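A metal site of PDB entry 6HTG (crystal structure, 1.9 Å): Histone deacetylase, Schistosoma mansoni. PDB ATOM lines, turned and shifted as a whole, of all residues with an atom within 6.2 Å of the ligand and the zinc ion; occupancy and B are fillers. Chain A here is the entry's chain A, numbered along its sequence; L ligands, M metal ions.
OH of Tyr 342 lies close to O3 of the ligand (3.4 Å).
A nitrogen (N1) of the ligand sits at hydrogen-bond distance from a ring nitrogen (NE2) of His 143 (2.8 Å).
A ring nitrogen (NE2) of His 142 lies close to an oxygen (O2) of the ligand (2.8 Å).
OD1 of Asp 286 is in hydrogen-bond range of N of Leu 188 (2.9 Å).
The side-chain amide nitrogen of Gln 282 is in hydrogen-bond range of the side-chain carboxylate of Asp 187 (3.2 Å).
The backbone NH of Tyr 342 sits at hydrogen-bond distance from the side-chain carboxylate of Asp 291, 3.0 Å away.
A ring nitrogen (NE2) of His 142 is in hydrogen-bond range of a ring nitrogen (NE2) of His 143 (3.2 Å).
N of His 143 sits at hydrogen-bond distance from SG of Cys 153 (3.5 Å).
A ring nitrogen (ND1) of His 142 lies close to the side-chain amide nitrogen (NE2) of Gln 282, 3.4 Å away.
A ring nitrogen (ND1) of His 293 lies within hydrogen-bond range of the side-chain carboxylate (OD1) of Asp 291, 2.8 Å away.
O of Gly 151 lies within hydrogen-bond range of SG of Cys 153 (3.6 Å).
Lys 21 touches the ligand.
Gly 151 touches the ligand (CA to C8, 3.95 Å).
Phe 217 touches the ligand.
CB of Pro 292 touches C3 of the ligand (3.8 Å).
His 293 touches the ligand.
Gly 340 touches the ligand.
Hydrophobic or aromatic side chains that line the ligand: His 142, His 143, His 189, Phe 217, Pro 292, His 293 and Tyr 342.
Within 4 Å of the ligand: Lys 21, His 142, His 143, Gly 151, Asp 187, His 189, Phe 217, Asp 286, Pro 292, His 293, Gly 340 and Tyr 342.
Of the 25 residues printed, 3 come within 4 Å of the zinc ion.
The nearest printed residue that does not touch the zinc ion is Gly 340 (4.04 Å).
The zinc ion is bound by the side-chain carboxylate of Asp 286 (1.9 Å), the side-chain carboxylate of Asp 187 (2.0 Å), a ring nitrogen (ND1) of His 189 (2.1 Å), an oxygen (O2) of the ligand (2.4 Å) and an oxygen (O1) of the ligand (2.4 Å).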
ATOM      1  N   LYS A  21     -13.802 -31.515  20.793  1.00  0.00           N
ATOM      2  CA  LYS A  21     -14.834 -31.337  21.813  1.00  0.00           C
ATOM      3  C   LYS A  21     -15.915 -32.410  21.745  1.00  0.00           C
ATOM      4  O   LYS A  21     -16.388 -32.889  22.786  1.00  0.00           O
ATOM      5  CB  LYS A  21     -15.473 -29.957  21.681  1.00  0.00           C
ATOM      6  CG  LYS A  21     -16.586 -29.716  22.681  1.00  0.00           C
ATOM      7  CD  LYS A  21     -17.051 -28.255  22.689  1.00  0.00           C
ATOM      8  CE  LYS A  21     -16.905 -27.597  24.067  1.00  0.00           C
ATOM      9  NZ  LYS A  21     -17.332 -26.153  24.058  1.00  0.00           N
ATOM     10  N   PHE A  22     -16.393 -32.747  20.542  1.00  0.00           N
ATOM     11  CA  PHE A  22     -17.524 -33.652  20.434  1.00  0.00           C
ATOM     12  C   PHE A  22     -17.134 -35.082  20.092  1.00  0.00           C
ATOM     13  O   PHE A  22     -18.012 -35.950  20.045  1.00  0.00           O
ATOM     14  CB  PHE A  22     -18.556 -33.100  19.440  1.00  0.00           C
ATOM     15  CG  PHE A  22     -19.300 -31.895  19.956  1.00  0.00           C
ATOM     16  CD1 PHE A  22     -20.303 -32.040  20.895  1.00  0.00           C
ATOM     17  CD2 PHE A  22     -18.942 -30.615  19.557  1.00  0.00           C
ATOM     18  CE1 PHE A  22     -20.973 -30.958  21.402  1.00  0.00           C
ATOM     19  CE2 PHE A  22     -19.608 -29.489  20.070  1.00  0.00           C
ATOM     20  CZ  PHE A  22     -20.628 -29.661  20.981  1.00  0.00           C
ATOM     21  N   ASP A 101     -12.114 -21.124  23.456  1.00  0.00           N
ATOM     22  CA  ASP A 101     -13.135 -22.166  23.344  1.00  0.00           C
ATOM     23  C   ASP A 101     -13.485 -22.530  21.907  1.00  0.00           C
ATOM     24  O   ASP A 101     -14.281 -23.461  21.709  1.00  0.00           O
ATOM     25  CB  ASP A 101     -14.416 -21.750  24.068  1.00  0.00           C
ATOM     26  CG  ASP A 101     -14.287 -21.813  25.569  1.00  0.00           C
ATOM     27  OD1 ASP A 101     -13.456 -22.616  26.053  1.00  0.00           O
ATOM     28  OD2 ASP A 101     -15.013 -21.072  26.267  1.00  0.00           O
ATOM     29  N   GLY A 140     -27.030 -27.862  14.247  1.00  0.00           N
ATOM     30  CA  GLY A 140     -27.544 -27.145  15.404  1.00  0.00           C
ATOM     31  C   GLY A 140     -26.586 -26.170  16.068  1.00  0.00           C
ATOM     32  O   GLY A 140     -26.741 -25.914  17.269  1.00  0.00           O
ATOM     33  N   HIS A 142     -25.763 -23.090  17.050  1.00  0.00           N
ATOM     34  CA  HIS A 142     -26.515 -21.843  17.079  1.00  0.00           C
ATOM     35  C   HIS A 142     -25.706 -20.623  17.514  1.00  0.00           C
ATOM     36  O   HIS A 142     -26.218 -19.498  17.411  1.00  0.00           O
ATOM     37  CB  HIS A 142     -27.764 -22.000  17.974  1.00  0.00           C
ATOM     38  CG  HIS A 142     -27.492 -22.496  19.357  1.00  0.00           C
ATOM     39  ND1 HIS A 142     -28.472 -22.541  20.332  1.00  0.00           N
ATOM     40  CD2 HIS A 142     -26.371 -22.983  19.933  1.00  0.00           C
ATOM     41  CE1 HIS A 142     -27.966 -23.049  21.443  1.00  0.00           C
ATOM     42  NE2 HIS A 142     -26.690 -23.302  21.235  1.00  0.00           N
ATOM     43  N   HIS A 143     -24.477 -20.792  18.008  1.00  0.00           N
ATOM     44  CA  HIS A 143     -23.764 -19.639  18.579  1.00  0.00           C
ATOM     45  C   HIS A 143     -22.916 -18.871  17.562  1.00  0.00           C
ATOM     46  O   HIS A 143     -22.552 -17.718  17.835  1.00  0.00           O
ATOM     47  CB  HIS A 143     -22.828 -20.083  19.720  1.00  0.00           C
ATOM     48  CG  HIS A 143     -23.544 -20.609  20.916  1.00  0.00           C
ATOM     49  ND1 HIS A 143     -24.587 -19.944  21.515  1.00  0.00           N
ATOM     50  CD2 HIS A 143     -23.337 -21.729  21.654  1.00  0.00           C
ATOM     51  CE1 HIS A 143     -25.010 -20.630  22.563  1.00  0.00           C
ATOM     52  NE2 HIS A 143     -24.266 -21.709  22.675  1.00  0.00           N
ATOM     53  N   SER A 150     -18.047 -18.909  18.142  1.00  0.00           N
ATOM     54  CA  SER A 150     -18.459 -18.786  19.537  1.00  0.00           C
ATOM     55  C   SER A 150     -18.979 -20.114  20.055  1.00  0.00           C
ATOM     56  O   SER A 150     -19.762 -20.774  19.363  1.00  0.00           O
ATOM     57  CB  SER A 150     -19.538 -17.710  19.685  1.00  0.00           C
ATOM     58  OG  SER A 150     -20.035 -17.691  21.017  1.00  0.00           O
ATOM     59  N   GLY A 151     -18.605 -20.479  21.268  1.00  0.00           N
ATOM     60  CA  GLY A 151     -19.195 -21.676  21.876  1.00  0.00           C
ATOM     61  C   GLY A 151     -18.970 -22.950  21.097  1.00  0.00           C
ATOM     62  O   GLY A 151     -19.848 -23.818  21.051  1.00  0.00           O
ATOM     63  N   PHE A 152     -17.794 -23.090  20.488  1.00  0.00           N
ATOM     64  CA  PHE A 152     -17.424 -24.214  19.607  1.00  0.00           C
ATOM     65  C   PHE A 152     -18.337 -24.306  18.402  1.00  0.00           C
ATOM     66  O   PHE A 152     -18.472 -25.386  17.808  1.00  0.00           O
ATOM     67  CB  PHE A 152     -17.378 -25.565  20.334  1.00  0.00           C
ATOM     68  CG  PHE A 152     -16.409 -26.561  19.686  1.00  0.00           C
ATOM     69  CD1 PHE A 152     -15.043 -26.516  19.982  1.00  0.00           C
ATOM     70  CD2 PHE A 152     -16.861 -27.515  18.749  1.00  0.00           C
ATOM     71  CE1 PHE A 152     -14.133 -27.392  19.380  1.00  0.00           C
ATOM     72  CE2 PHE A 152     -15.969 -28.378  18.153  1.00  0.00           C
ATOM     73  CZ  PHE A 152     -14.593 -28.327  18.480  1.00  0.00           C
ATOM     74  N   CYS A 153     -18.996 -23.200  18.047  1.00  0.00           N
ATOM     75  CA  CYS A 153     -19.732 -23.060  16.812  1.00  0.00           C
ATOM     76  C   CYS A 153     -18.888 -22.220  15.867  1.00  0.00           C
ATOM     77  O   CYS A 153     -18.591 -21.063  16.173  1.00  0.00           O
ATOM     78  CB  CYS A 153     -21.076 -22.376  17.043  1.00  0.00           C
ATOM     79  SG  CYS A 153     -22.079 -23.331  18.228  1.00  0.00           S
ATOM     80  N   ASP A 187     -31.960 -25.916  23.518  1.00  0.00           N
ATOM     81  CA  ASP A 187     -30.654 -26.036  24.138  1.00  0.00           C
ATOM     82  C   ASP A 187     -30.621 -25.361  25.520  1.00  0.00           C
ATOM     83  O   ASP A 187     -31.386 -24.435  25.806  1.00  0.00           O
ATOM     84  CB  ASP A 187     -29.622 -25.413  23.187  1.00  0.00           C
ATOM     85  CG  ASP A 187     -28.192 -25.861  23.481  1.00  0.00           C
ATOM     86  OD1 ASP A 187     -27.664 -26.780  22.802  1.00  0.00           O
ATOM     87  OD2 ASP A 187     -27.585 -25.252  24.383  1.00  0.00           O
ATOM     88  N   LEU A 188     -29.757 -25.886  26.394  1.00  0.00           N
ATOM     89  CA  LEU A 188     -29.497 -25.238  27.689  1.00  0.00           C
ATOM     90  C   LEU A 188     -29.084 -23.789  27.521  1.00  0.00           C
ATOM     91  O   LEU A 188     -29.415 -22.952  28.354  1.00  0.00           O
ATOM     92  CB  LEU A 188     -28.418 -25.996  28.465  1.00  0.00           C
ATOM     93  CG  LEU A 188     -28.016 -25.458  29.844  1.00  0.00           C
ATOM     94  CD1 LEU A 188     -29.199 -25.544  30.852  1.00  0.00           C
ATOM     95  CD2 LEU A 188     -26.806 -26.256  30.320  1.00  0.00           C
ATOM     96  N   HIS A 189     -28.378 -23.478  26.442  1.00  0.00           N
ATOM     97  CA  HIS A 189     -27.820 -22.147  26.227  1.00  0.00           C
ATOM     98  C   HIS A 189     -28.709 -21.327  25.317  1.00  0.00           C
ATOM     99  O   HIS A 189     -29.399 -21.859  24.446  1.00  0.00           O
ATOM    100  CB  HIS A 189     -26.404 -22.235  25.657  1.00  0.00           C
ATOM    101  CG  HIS A 189     -25.448 -22.970  26.545  1.00  0.00           C
ATOM    102  ND1 HIS A 189     -25.215 -24.314  26.424  1.00  0.00           N
ATOM    103  CD2 HIS A 189     -24.714 -22.545  27.599  1.00  0.00           C
ATOM    104  CE1 HIS A 189     -24.349 -24.698  27.358  1.00  0.00           C
ATOM    105  NE2 HIS A 189     -24.036 -23.643  28.080  1.00  0.00           N
ATOM    106  N   HIS A 190     -28.680 -20.024  25.543  1.00  0.00           N
ATOM    107  CA  HIS A 190     -29.381 -19.083  24.693  1.00  0.00           C
ATOM    108  C   HIS A 190     -28.887 -19.179  23.243  1.00  0.00           C
ATOM    109  O   HIS A 190     -27.681 -19.143  22.998  1.00  0.00           O
ATOM    110  CB  HIS A 190     -29.151 -17.669  25.183  1.00  0.00           C
ATOM    111  CG  HIS A 190     -29.767 -16.630  24.301  1.00  0.00           C
ATOM    112  ND1 HIS A 190     -29.069 -15.571  23.790  1.00  0.00           N
ATOM    113  CD2 HIS A 190     -31.026 -16.541  23.808  1.00  0.00           C
ATOM    114  CE1 HIS A 190     -29.880 -14.830  23.050  1.00  0.00           C
ATOM    115  NE2 HIS A 190     -31.071 -15.403  23.035  1.00  0.00           N
ATOM    116  N   PHE A 217     -22.668 -18.664  30.188  1.00  0.00           N
ATOM    117  CA  PHE A 217     -22.560 -18.472  28.734  1.00  0.00           C
ATOM    118  C   PHE A 217     -23.931 -18.527  28.025  1.00  0.00           C
ATOM    119  O   PHE A 217     -24.752 -19.363  28.381  1.00  0.00           O
ATOM    120  CB  PHE A 217     -21.637 -19.563  28.160  1.00  0.00           C
ATOM    121  CG  PHE A 217     -21.335 -19.394  26.708  1.00  0.00           C
ATOM    122  CD1 PHE A 217     -20.244 -18.629  26.303  1.00  0.00           C
ATOM    123  CD2 PHE A 217     -22.121 -19.989  25.734  1.00  0.00           C
ATOM    124  CE1 PHE A 217     -19.934 -18.465  24.952  1.00  0.00           C
ATOM    125  CE2 PHE A 217     -21.828 -19.816  24.367  1.00  0.00           C
ATOM    126  CZ  PHE A 217     -20.723 -19.061  23.992  1.00  0.00           C
ATOM    127  N   GLN A 282     -33.890 -26.631  17.340  1.00  0.00           N
ATOM    128  CA  GLN A 282     -32.610 -27.052  17.871  1.00  0.00           C
ATOM    129  C   GLN A 282     -32.870 -27.858  19.142  1.00  0.00           C
ATOM    130  O   GLN A 282     -33.572 -27.388  20.043  1.00  0.00           O
ATOM    131  CB  GLN A 282     -31.735 -25.828  18.145  1.00  0.00           C
ATOM    132  CG  GLN A 282     -30.224 -26.011  18.151  1.00  0.00           C
ATOM    133  CD  GLN A 282     -29.727 -26.247  19.551  1.00  0.00           C
ATOM    134  OE1 GLN A 282     -30.476 -26.693  20.398  1.00  0.00           O
ATOM    135  NE2 GLN A 282     -28.451 -25.942  19.797  1.00  0.00           N
ATOM    136  N   GLY A 284     -30.592 -29.289  21.446  1.00  0.00           N
ATOM    137  CA  GLY A 284     -29.440 -29.445  22.325  1.00  0.00           C
ATOM    138  C   GLY A 284     -29.775 -30.229  23.579  1.00  0.00           C
ATOM    139  O   GLY A 284     -30.768 -29.950  24.250  1.00  0.00           O
ATOM    140  N   ASP A 286     -28.071 -30.644  26.363  1.00  0.00           N
ATOM    141  CA  ASP A 286     -27.394 -30.278  27.603  1.00  0.00           C
ATOM    142  C   ASP A 286     -28.355 -29.907  28.723  1.00  0.00           C
ATOM    143  O   ASP A 286     -27.872 -29.597  29.808  1.00  0.00           O
ATOM    144  CB  ASP A 286     -26.369 -29.160  27.400  1.00  0.00           C
ATOM    145  CG  ASP A 286     -26.761 -28.120  26.362  1.00  0.00           C
ATOM    146  OD1 ASP A 286     -27.902 -28.025  25.896  1.00  0.00           O
ATOM    147  OD2 ASP A 286     -25.836 -27.346  26.023  1.00  0.00           O
ATOM    148  N   ASP A 291     -26.314 -34.315  32.156  1.00  0.00           N
ATOM    149  CA  ASP A 291     -25.287 -33.575  31.419  1.00  0.00           C
ATOM    150  C   ASP A 291     -24.267 -33.013  32.408  1.00  0.00           C
ATOM    151  O   ASP A 291     -24.625 -32.665  33.534  1.00  0.00           O
ATOM    152  CB  ASP A 291     -25.937 -32.459  30.598  1.00  0.00           C
ATOM    153  CG  ASP A 291     -24.920 -31.743  29.706  1.00  0.00           C
ATOM    154  OD1 ASP A 291     -24.263 -30.823  30.204  1.00  0.00           O
ATOM    155  OD2 ASP A 291     -24.780 -32.123  28.509  1.00  0.00           O
ATOM    156  N   PRO A 292     -22.969 -32.978  32.027  1.00  0.00           N
ATOM    157  CA  PRO A 292     -21.948 -32.409  32.937  1.00  0.00           C
ATOM    158  C   PRO A 292     -22.253 -30.989  33.422  1.00  0.00           C
ATOM    159  O   PRO A 292     -21.790 -30.618  34.504  1.00  0.00           O
ATOM    160  CB  PRO A 292     -20.661 -32.420  32.094  1.00  0.00           C
ATOM    161  CG  PRO A 292     -20.929 -33.227  30.903  1.00  0.00           C
ATOM    162  CD  PRO A 292     -22.399 -33.467  30.762  1.00  0.00           C
ATOM    163  N   HIS A 293     -22.988 -30.171  32.654  1.00  0.00           N
ATOM    164  CA  HIS A 293     -23.347 -28.853  33.183  1.00  0.00           C
ATOM    165  C   HIS A 293     -24.142 -28.957  34.472  1.00  0.00           C
ATOM    166  O   HIS A 293     -24.061 -28.047  35.319  1.00  0.00           O
ATOM    167  CB  HIS A 293     -24.175 -28.050  32.166  1.00  0.00           C
ATOM    168  CG  HIS A 293     -23.381 -27.529  31.012  1.00  0.00           C
ATOM    169  ND1 HIS A 293     -22.978 -28.332  29.971  1.00  0.00           N
ATOM    170  CD2 HIS A 293     -22.941 -26.281  30.723  1.00  0.00           C
ATOM    171  CE1 HIS A 293     -22.316 -27.608  29.098  1.00  0.00           C
ATOM    172  NE2 HIS A 293     -22.270 -26.361  29.522  1.00  0.00           N
ATOM    173  N   GLY A 339     -27.166 -30.143  18.728  1.00  0.00           N
ATOM    174  CA  GLY A 339     -26.555 -28.991  19.339  1.00  0.00           C
ATOM    175  C   GLY A 339     -25.747 -29.444  20.529  1.00  0.00           C
ATOM    176  O   GLY A 339     -25.017 -30.434  20.418  1.00  0.00           O
ATOM    177  N   GLY A 340     -25.894 -28.761  21.658  1.00  0.00           N
ATOM    178  CA  GLY A 340     -25.180 -29.140  22.870  1.00  0.00           C
ATOM    179  C   GLY A 340     -25.473 -30.584  23.290  1.00  0.00           C
ATOM    180  O   GLY A 340     -26.347 -31.262  22.761  1.00  0.00           O
ATOM    181  N   GLY A 341     -24.681 -31.039  24.261  1.00  0.00           N
ATOM    182  CA  GLY A 341     -24.863 -32.375  24.800  1.00  0.00           C
ATOM    183  C   GLY A 341     -23.537 -33.059  25.042  1.00  0.00           C
ATOM    184  O   GLY A 341     -22.930 -33.621  24.121  1.00  0.00           O
ATOM    185  N   TYR A 342     -23.061 -33.032  26.281  1.00  0.00           N
ATOM    186  CA  TYR A 342     -21.687 -33.383  26.612  1.00  0.00           C
ATOM    187  C   TYR A 342     -21.588 -34.703  27.359  1.00  0.00           C
ATOM    188  O   TYR A 342     -20.472 -35.150  27.672  1.00  0.00           O
ATOM    189  CB  TYR A 342     -21.075 -32.205  27.378  1.00  0.00           C
ATOM    190  CG  TYR A 342     -21.236 -30.989  26.478  1.00  0.00           C
ATOM    191  CD1 TYR A 342     -20.338 -30.788  25.427  1.00  0.00           C
ATOM    192  CD2 TYR A 342     -22.331 -30.143  26.583  1.00  0.00           C
ATOM    193  CE1 TYR A 342     -20.503 -29.748  24.543  1.00  0.00           C
ATOM    194  CE2 TYR A 342     -22.510 -29.089  25.691  1.00  0.00           C
ATOM    195  CZ  TYR A 342     -21.579 -28.899  24.680  1.00  0.00           C
ATOM    196  OH  TYR A 342     -21.711 -27.857  23.802  1.00  0.00           O
HETATM  197  N1  LIG L   1     -23.695 -24.340  23.454  1.00  0.00           N
HETATM  198  C1  LIG L   1     -23.035 -25.186  24.228  1.00  0.00           C
HETATM  199  O1  LIG L   1     -23.457 -26.317  24.467  1.00  0.00           O
HETATM  200  C2  LIG L   1     -21.766 -24.686  24.855  1.00  0.00           C
HETATM  201  C3  LIG L   1     -18.721 -29.309  31.076  1.00  0.00           C
HETATM  202  C4  LIG L   1     -18.422 -29.872  29.865  1.00  0.00           C
HETATM  203  C5  LIG L   1     -18.557 -29.135  28.699  1.00  0.00           C
HETATM  204  C6  LIG L   1     -21.024 -25.518  25.695  1.00  0.00           C
HETATM  205  C7  LIG L   1     -21.401 -23.354  24.715  1.00  0.00           C
HETATM  206  C8  LIG L   1     -20.357 -22.835  25.472  1.00  0.00           C
HETATM  207  C9  LIG L   1     -19.668 -23.656  26.348  1.00  0.00           C
HETATM  208  C10 LIG L   1     -19.953 -25.016  26.447  1.00  0.00           C
HETATM  209  C11 LIG L   1     -19.313 -27.161  27.438  1.00  0.00           C
HETATM  210  C12 LIG L   1     -19.003 -27.810  28.752  1.00  0.00           C
HETATM  211  C13 LIG L   1     -19.262 -27.244  29.992  1.00  0.00           C
HETATM  212  C14 LIG L   1     -19.133 -27.999  31.148  1.00  0.00           C
HETATM  213  N2  LIG L   1     -19.234 -25.819  27.381  1.00  0.00           N
HETATM  214  O2  LIG L   1     -24.959 -24.688  22.989  1.00  0.00           O
HETATM  215  O3  LIG L   1     -19.554 -27.849  26.466  1.00  0.00           O
HETATM  216 CL1  LIG L   1     -18.439 -22.957  27.359  1.00  0.00          CL
HETATM  217 ZN    ZN M   1     -25.762 -25.729  24.964  1.00  0.00          ZN
